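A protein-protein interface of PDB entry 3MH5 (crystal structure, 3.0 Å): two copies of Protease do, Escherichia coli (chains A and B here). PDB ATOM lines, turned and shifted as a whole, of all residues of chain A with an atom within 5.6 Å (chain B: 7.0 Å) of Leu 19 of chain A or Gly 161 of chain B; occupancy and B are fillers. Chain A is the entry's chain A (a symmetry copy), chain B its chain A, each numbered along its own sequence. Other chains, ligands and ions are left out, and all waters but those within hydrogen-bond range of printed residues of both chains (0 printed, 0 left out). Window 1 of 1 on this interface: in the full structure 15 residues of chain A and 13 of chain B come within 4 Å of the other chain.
No position is printed for both chains.
The side-chain carboxylate of Glu 20 of chain A is in salt-bridge range of the guanidinium group of Arg 159 of chain B (2.9 Å).
The backbone carbonyl oxygen (O) of Val 177 of chain A sits at hydrogen-bond distance from the side-chain hydroxyl (OG) of Ser 183 of chain B, 3.0 Å away.
N of Leu 15 of chain A lies within hydrogen-bond range of O of Gly 161 of chain B (3.2 Å).
OD1 of Asp 162 of chain B is in hydrogen-bond range of OG of Ser 14 of chain A, 2.7 Å away.
N of Arg 159 of chain B lies within hydrogen-bond range of OD2 of Asp 162 of chain B.
OG of Ser 14 of chain A is in hydrogen-bond range of N of Ala 16 of chain A (2.9 Å).
N of Val 182 of chain B lies within hydrogen-bond range of O of Asp 162 of chain B, 2.6 Å away.
The backbone NH of Val 182 of chain B lies close to the backbone carbonyl oxygen of Val 160 of chain B, at 3.1 Å.
Ser 14 of chain A touches Gly 161 of chain B (OG to O, 3.6 Å).
Ser 14 of chain A touches Tyr 163 of chain B.
Leu 15 of chain A touches Tyr 163 of chain B.
CD1 of Leu 15 of chain A touches CG2 of Ile 181 of chain B, 3.96 Å away.
Ala 16 of chain A touches Gly 161 of chain B (N to CA, 3.7 Å).
OD1 of Asp 162 of chain B touches CB of Ala 16 of chain A (3.9 Å).
Pro 17 of chain A touches Arg 159 of chain B.
CA of Gly 161 of chain B touches CD1 of Leu 19 of chain A, at 3.5 Å.
CG2 of Val 177 of chain A touches CG1 of Val 160 of chain B, 3.5 Å away.
Val 177 of chain A touches Ile 181 of chain B (O to CD1, 3.6 Å).
Of the 14 printed residues of chain A, 7 touch a printed residue of chain B.
Printed residues of chain A that touch a printed residue of chain B: Ser 14, Leu 15, Ala 16, Pro 17, Leu 19, Glu 20 and Val 177.
Hydrophobic or aromatic side chains of chain A within 4 Å of the printed part of chain B: Leu 15, Ala 16, Pro 17, Leu 19 and Val 177.
Along chain A the printed residues that touch a printed residue of chain B span positions 14 to 177.
Of the printed residues of chain B, Leu 19 of chain A touches Gly 161 (3.5 Å).
Printed residues of chain B within 4 Å of Glu 20 of chain A: Arg 159 (2.9 Å).
Pro 24 of chain A touches none of the printed residues of chain B.
Of the printed residues of chain A, Arg 159 of chain B touches Ala 16, Pro 17 and Glu 20.
Of the printed residues of chain A, Val 160 of chain B touches Val 177.
Gly 161 of chain B touches just these residues of chain A: Ser 14, Leu 15, Ala 16 and Leu 19.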
ATOM      1  N   SER A  14     -16.018  31.718 -25.454  1.00  0.00           N
ATOM      2  CA  SER A  14     -14.842  30.978 -25.018  1.00  0.00           C
ATOM      3  C   SER A  14     -14.514  31.246 -23.554  1.00  0.00           C
ATOM      4  O   SER A  14     -14.832  32.309 -23.007  1.00  0.00           O
ATOM      5  CB  SER A  14     -13.636  31.343 -25.888  1.00  0.00           C
ATOM      6  OG  SER A  14     -12.435  30.839 -25.336  1.00  0.00           O
ATOM      7  N   LEU A  15     -13.876  30.267 -22.925  1.00  0.00           N
ATOM      8  CA  LEU A  15     -13.491  30.369 -21.528  1.00  0.00           C
ATOM      9  C   LEU A  15     -12.104  31.028 -21.446  1.00  0.00           C
ATOM     10  O   LEU A  15     -11.645  31.433 -20.372  1.00  0.00           O
ATOM     11  CB  LEU A  15     -13.463  28.963 -20.917  1.00  0.00           C
ATOM     12  CG  LEU A  15     -14.735  28.103 -21.025  1.00  0.00           C
ATOM     13  CD1 LEU A  15     -14.385  26.634 -20.854  1.00  0.00           C
ATOM     14  CD2 LEU A  15     -15.746  28.509 -19.979  1.00  0.00           C
ATOM     15  N   ALA A  16     -11.454  31.145 -22.601  1.00  0.00           N
ATOM     16  CA  ALA A  16     -10.121  31.732 -22.684  1.00  0.00           C
ATOM     17  C   ALA A  16     -10.002  33.033 -21.907  1.00  0.00           C
ATOM     18  O   ALA A  16      -9.056  33.216 -21.141  1.00  0.00           O
ATOM     19  CB  ALA A  16      -9.749  31.950 -24.115  1.00  0.00           C
ATOM     20  N   PRO A  17     -10.944  33.965 -22.108  1.00  0.00           N
ATOM     21  CA  PRO A  17     -10.840  35.215 -21.357  1.00  0.00           C
ATOM     22  C   PRO A  17     -10.691  34.991 -19.844  1.00  0.00           C
ATOM     23  O   PRO A  17      -9.697  35.406 -19.252  1.00  0.00           O
ATOM     24  CB  PRO A  17     -12.123  35.941 -21.743  1.00  0.00           C
ATOM     25  CG  PRO A  17     -12.265  35.556 -23.189  1.00  0.00           C
ATOM     26  CD  PRO A  17     -11.958  34.071 -23.174  1.00  0.00           C
ATOM     27  N   MET A  18     -11.653  34.314 -19.222  1.00  0.00           N
ATOM     28  CA  MET A  18     -11.574  34.091 -17.782  1.00  0.00           C
ATOM     29  C   MET A  18     -10.354  33.259 -17.376  1.00  0.00           C
ATOM     30  O   MET A  18      -9.754  33.498 -16.329  1.00  0.00           O
ATOM     31  CB  MET A  18     -12.859  33.423 -17.264  1.00  0.00           C
ATOM     32  CG  MET A  18     -12.846  31.906 -17.299  1.00  0.00           C
ATOM     33  SD  MET A  18     -12.116  31.140 -15.836  1.00  0.00           S
ATOM     34  CE  MET A  18     -13.221  29.709 -15.631  1.00  0.00           C
ATOM     35  N   LEU A  19      -9.981  32.282 -18.192  1.00  0.00           N
ATOM     36  CA  LEU A  19      -8.831  31.462 -17.838  1.00  0.00           C
ATOM     37  C   LEU A  19      -7.584  32.316 -17.832  1.00  0.00           C
ATOM     38  O   LEU A  19      -6.645  32.039 -17.086  1.00  0.00           O
ATOM     39  CB  LEU A  19      -8.653  30.288 -18.809  1.00  0.00           C
ATOM     40  CG  LEU A  19      -9.670  29.141 -18.695  1.00  0.00           C
ATOM     41  CD1 LEU A  19      -9.429  28.102 -19.781  1.00  0.00           C
ATOM     42  CD2 LEU A  19      -9.565  28.505 -17.325  1.00  0.00           C
ATOM     43  N   GLU A  20      -7.570  33.363 -18.658  1.00  0.00           N
ATOM     44  CA  GLU A  20      -6.409  34.242 -18.727  1.00  0.00           C
ATOM     45  C   GLU A  20      -6.223  34.991 -17.409  1.00  0.00           C
ATOM     46  O   GLU A  20      -5.114  35.409 -17.071  1.00  0.00           O
ATOM     47  CB  GLU A  20      -6.545  35.214 -19.900  1.00  0.00           C
ATOM     48  CG  GLU A  20      -6.408  34.531 -21.259  1.00  0.00           C
ATOM     49  CD  GLU A  20      -6.238  35.515 -22.407  1.00  0.00           C
ATOM     50  OE1 GLU A  20      -5.310  36.347 -22.337  1.00  0.00           O
ATOM     51  OE2 GLU A  20      -7.023  35.450 -23.382  1.00  0.00           O
ATOM     52  N   LYS A  21      -7.308  35.134 -16.654  1.00  0.00           N
ATOM     53  CA  LYS A  21      -7.251  35.808 -15.368  1.00  0.00           C
ATOM     54  C   LYS A  21      -6.877  34.812 -14.263  1.00  0.00           C
ATOM     55  O   LYS A  21      -6.110  35.139 -13.359  1.00  0.00           O
ATOM     56  CB  LYS A  21      -8.606  36.462 -15.067  1.00  0.00           C
ATOM     57  CG  LYS A  21      -8.682  37.175 -13.723  1.00  0.00           C
ATOM     58  CD  LYS A  21      -9.865  38.143 -13.670  1.00  0.00           C
ATOM     59  CE  LYS A  21     -11.204  37.443 -13.842  1.00  0.00           C
ATOM     60  NZ  LYS A  21     -11.524  36.565 -12.684  1.00  0.00           N
ATOM     61  N   VAL A  22      -7.399  33.592 -14.361  1.00  0.00           N
ATOM     62  CA  VAL A  22      -7.157  32.533 -13.372  1.00  0.00           C
ATOM     63  C   VAL A  22      -5.774  31.870 -13.383  1.00  0.00           C
ATOM     64  O   VAL A  22      -5.160  31.660 -12.339  1.00  0.00           O
ATOM     65  CB  VAL A  22      -8.204  31.400 -13.521  1.00  0.00           C
ATOM     66  CG1 VAL A  22      -7.870  30.254 -12.582  1.00  0.00           C
ATOM     67  CG2 VAL A  22      -9.600  31.939 -13.235  1.00  0.00           C
ATOM     68  N   MET A  23      -5.283  31.534 -14.562  1.00  0.00           N
ATOM     69  CA  MET A  23      -4.004  30.850 -14.674  1.00  0.00           C
ATOM     70  C   MET A  23      -2.847  31.355 -13.824  1.00  0.00           C
ATOM     71  O   MET A  23      -2.045  30.564 -13.339  1.00  0.00           O
ATOM     72  CB  MET A  23      -3.589  30.782 -16.141  1.00  0.00           C
ATOM     73  CG  MET A  23      -4.489  29.867 -16.958  1.00  0.00           C
ATOM     74  SD  MET A  23      -4.570  28.192 -16.228  1.00  0.00           S
ATOM     75  CE  MET A  23      -2.914  27.632 -16.602  1.00  0.00           C
ATOM     76  N   PRO A  24      -2.733  32.674 -13.636  1.00  0.00           N
ATOM     77  CA  PRO A  24      -1.623  33.180 -12.818  1.00  0.00           C
ATOM     78  C   PRO A  24      -1.623  32.652 -11.371  1.00  0.00           C
ATOM     79  O   PRO A  24      -0.594  32.674 -10.690  1.00  0.00           O
ATOM     80  CB  PRO A  24      -1.823  34.687 -12.887  1.00  0.00           C
ATOM     81  CG  PRO A  24      -2.418  34.871 -14.272  1.00  0.00           C
ATOM     82  CD  PRO A  24      -3.437  33.777 -14.316  1.00  0.00           C
ATOM     83  N   VAL A 165     -14.979  24.392 -14.229  1.00  0.00           N
ATOM     84  CA  VAL A 165     -13.797  24.169 -15.050  1.00  0.00           C
ATOM     85  C   VAL A 165     -12.697  23.636 -14.149  1.00  0.00           C
ATOM     86  O   VAL A 165     -12.464  24.157 -13.056  1.00  0.00           O
ATOM     87  CB  VAL A 165     -13.312  25.459 -15.727  1.00  0.00           C
ATOM     88  CG1 VAL A 165     -12.003  25.204 -16.462  1.00  0.00           C
ATOM     89  CG2 VAL A 165     -14.349  25.944 -16.717  1.00  0.00           C
ATOM     90  N   ILE A 167      -8.641  22.668 -13.702  1.00  0.00           N
ATOM     91  CA  ILE A 167      -7.302  22.993 -14.186  1.00  0.00           C
ATOM     92  C   ILE A 167      -6.301  22.075 -13.503  1.00  0.00           C
ATOM     93  O   ILE A 167      -6.364  21.902 -12.294  1.00  0.00           O
ATOM     94  CB  ILE A 167      -6.954  24.456 -13.853  1.00  0.00           C
ATOM     95  CG1 ILE A 167      -7.995  25.381 -14.484  1.00  0.00           C
ATOM     96  CG2 ILE A 167      -5.551  24.787 -14.350  1.00  0.00           C
ATOM     97  CD1 ILE A 167      -7.915  26.776 -13.987  1.00  0.00           C
ATOM     98  N   VAL A 177      -6.885  22.153 -19.174  1.00  0.00           N
ATOM     99  CA  VAL A 177      -8.181  22.633 -18.734  1.00  0.00           C
ATOM    100  C   VAL A 177      -9.328  21.788 -19.288  1.00  0.00           C
ATOM    101  O   VAL A 177      -9.332  21.432 -20.462  1.00  0.00           O
ATOM    102  CB  VAL A 177      -8.381  24.105 -19.162  1.00  0.00           C
ATOM    103  CG1 VAL A 177      -9.705  24.633 -18.633  1.00  0.00           C
ATOM    104  CG2 VAL A 177      -7.236  24.950 -18.638  1.00  0.00           C
ATOM    105  N   ARG B 159      -6.697  28.948 -28.519  1.00  0.00           N
ATOM    106  CA  ARG B 159      -6.513  29.211 -27.095  1.00  0.00           C
ATOM    107  C   ARG B 159      -7.132  28.031 -26.341  1.00  0.00           C
ATOM    108  O   ARG B 159      -8.052  27.390 -26.842  1.00  0.00           O
ATOM    109  CB  ARG B 159      -7.205  30.524 -26.702  1.00  0.00           C
ATOM    110  CG  ARG B 159      -6.555  31.769 -27.284  1.00  0.00           C
ATOM    111  CD  ARG B 159      -7.125  33.036 -26.667  1.00  0.00           C
ATOM    112  NE  ARG B 159      -8.547  33.210 -26.974  1.00  0.00           N
ATOM    113  CZ  ARG B 159      -9.307  34.207 -26.512  1.00  0.00           C
ATOM    114  NH1 ARG B 159      -8.784  35.137 -25.712  1.00  0.00           N
ATOM    115  NH2 ARG B 159     -10.596  34.268 -26.842  1.00  0.00           N
ATOM    116  N   VAL B 160      -6.640  27.741 -25.144  1.00  0.00           N
ATOM    117  CA  VAL B 160      -7.168  26.607 -24.400  1.00  0.00           C
ATOM    118  C   VAL B 160      -8.672  26.612 -24.102  1.00  0.00           C
ATOM    119  O   VAL B 160      -9.388  25.710 -24.541  1.00  0.00           O
ATOM    120  CB  VAL B 160      -6.352  26.383 -23.107  1.00  0.00           C
ATOM    121  CG1 VAL B 160      -7.186  25.677 -22.056  1.00  0.00           C
ATOM    122  CG2 VAL B 160      -5.127  25.536 -23.443  1.00  0.00           C
ATOM    123  N   GLY B 161      -9.174  27.607 -23.387  1.00  0.00           N
ATOM    124  CA  GLY B 161     -10.602  27.599 -23.091  1.00  0.00           C
ATOM    125  C   GLY B 161     -11.573  27.510 -24.268  1.00  0.00           C
ATOM    126  O   GLY B 161     -12.785  27.502 -24.064  1.00  0.00           O
ATOM    127  N   ASP B 162     -11.048  27.433 -25.488  1.00  0.00           N
ATOM    128  CA  ASP B 162     -11.857  27.375 -26.710  1.00  0.00           C
ATOM    129  C   ASP B 162     -12.715  26.126 -26.918  1.00  0.00           C
ATOM    130  O   ASP B 162     -12.268  24.996 -26.690  1.00  0.00           O
ATOM    131  CB  ASP B 162     -10.950  27.553 -27.927  1.00  0.00           C
ATOM    132  CG  ASP B 162     -10.484  28.982 -28.103  1.00  0.00           C
ATOM    133  OD1 ASP B 162     -10.726  29.808 -27.195  1.00  0.00           O
ATOM    134  OD2 ASP B 162      -9.872  29.278 -29.154  1.00  0.00           O
ATOM    135  N   TYR B 163     -13.947  26.340 -27.375  1.00  0.00           N
ATOM    136  CA  TYR B 163     -14.861  25.230 -27.623  1.00  0.00           C
ATOM    137  C   TYR B 163     -14.559  24.551 -28.942  1.00  0.00           C
ATOM    138  O   TYR B 163     -14.379  25.212 -29.964  1.00  0.00           O
ATOM    139  CB  TYR B 163     -16.314  25.703 -27.648  1.00  0.00           C
ATOM    140  CG  TYR B 163     -16.785  26.276 -26.345  1.00  0.00           C
ATOM    141  CD1 TYR B 163     -16.738  27.648 -26.108  1.00  0.00           C
ATOM    142  CD2 TYR B 163     -17.246  25.446 -25.333  1.00  0.00           C
ATOM    143  CE1 TYR B 163     -17.139  28.178 -24.895  1.00  0.00           C
ATOM    144  CE2 TYR B 163     -17.648  25.966 -24.115  1.00  0.00           C
ATOM    145  CZ  TYR B 163     -17.589  27.332 -23.900  1.00  0.00           C
ATOM    146  OH  TYR B 163     -17.980  27.846 -22.686  1.00  0.00           O
ATOM    147  N   THR B 164     -14.535  23.225 -28.908  1.00  0.00           N
ATOM    148  CA  THR B 164     -14.258  22.425 -30.085  1.00  0.00           C
ATOM    149  C   THR B 164     -15.327  21.343 -30.266  1.00  0.00           C
ATOM    150  O   THR B 164     -16.065  21.020 -29.330  1.00  0.00           O
ATOM    151  CB  THR B 164     -12.884  21.750 -29.946  1.00  0.00           C
ATOM    152  OG1 THR B 164     -12.895  20.876 -28.811  1.00  0.00           O
ATOM    153  CG2 THR B 164     -11.801  22.789 -29.739  1.00  0.00           C
ATOM    154  N   GLY B 180     -16.433  19.672 -26.629  1.00  0.00           N
ATOM    155  CA  GLY B 180     -15.506  19.864 -25.527  1.00  0.00           C
ATOM    156  C   GLY B 180     -14.831  21.217 -25.665  1.00  0.00           C
ATOM    157  O   GLY B 180     -15.421  22.154 -26.215  1.00  0.00           O
ATOM    158  N   ILE B 181     -13.608  21.338 -25.156  1.00  0.00           N
ATOM    159  CA  ILE B 181     -12.846  22.584 -25.264  1.00  0.00           C
ATOM    160  C   ILE B 181     -11.391  22.217 -25.484  1.00  0.00           C
ATOM    161  O   ILE B 181     -11.015  21.058 -25.317  1.00  0.00           O
ATOM    162  CB  ILE B 181     -12.899  23.440 -23.978  1.00  0.00           C
ATOM    163  CG1 ILE B 181     -12.282  22.671 -22.811  1.00  0.00           C
ATOM    164  CG2 ILE B 181     -14.320  23.844 -23.666  1.00  0.00           C
ATOM    165  CD1 ILE B 181     -11.919  23.554 -21.657  1.00  0.00           C
ATOM    166  N   VAL B 182     -10.571  23.198 -25.850  1.00  0.00           N
ATOM    167  CA  VAL B 182      -9.147  22.941 -26.051  1.00  0.00           C
ATOM    168  C   VAL B 182      -8.517  22.797 -24.665  1.00  0.00           C
ATOM    169  O   VAL B 182      -8.446  23.758 -23.907  1.00  0.00           O
ATOM    170  CB  VAL B 182      -8.434  24.106 -26.787  1.00  0.00           C
ATOM    171  CG1 VAL B 182      -6.995  23.704 -27.104  1.00  0.00           C
ATOM    172  CG2 VAL B 182      -9.199  24.489 -28.057  1.00  0.00           C
ATOM    173  N   SER B 183      -8.066  21.596 -24.327  1.00  0.00           N
ATOM    174  CA  SER B 183      -7.469  21.386 -23.014  1.00  0.00           C
ATOM    175  C   SER B 183      -6.060  21.944 -22.933  1.00  0.00           C
ATOM    176  O   SER B 183      -5.754  22.752 -22.057  1.00  0.00           O
ATOM    177  CB  SER B 183      -7.458  19.897 -22.676  1.00  0.00           C
ATOM    178  OG  SER B 183      -8.781  19.389 -22.641  1.00  0.00           O
ATOM    179  N   LEU B 185      -2.466  23.162 -25.504  1.00  0.00           N
ATOM    180  CA  LEU B 185      -1.939  23.520 -26.813  1.00  0.00           C
ATOM    181  C   LEU B 185      -0.432  23.317 -26.874  1.00  0.00           C
ATOM    182  O   LEU B 185       0.058  22.202 -26.693  1.00  0.00           O
ATOM    183  CB  LEU B 185      -2.265  24.977 -27.135  1.00  0.00           C
ATOM    184  CG  LEU B 185      -3.688  25.323 -27.578  1.00  0.00           C
ATOM    185  CD1 LEU B 185      -3.802  26.833 -27.699  1.00  0.00           C
ATOM    186  CD2 LEU B 185      -4.022  24.642 -28.913  1.00  0.00           C
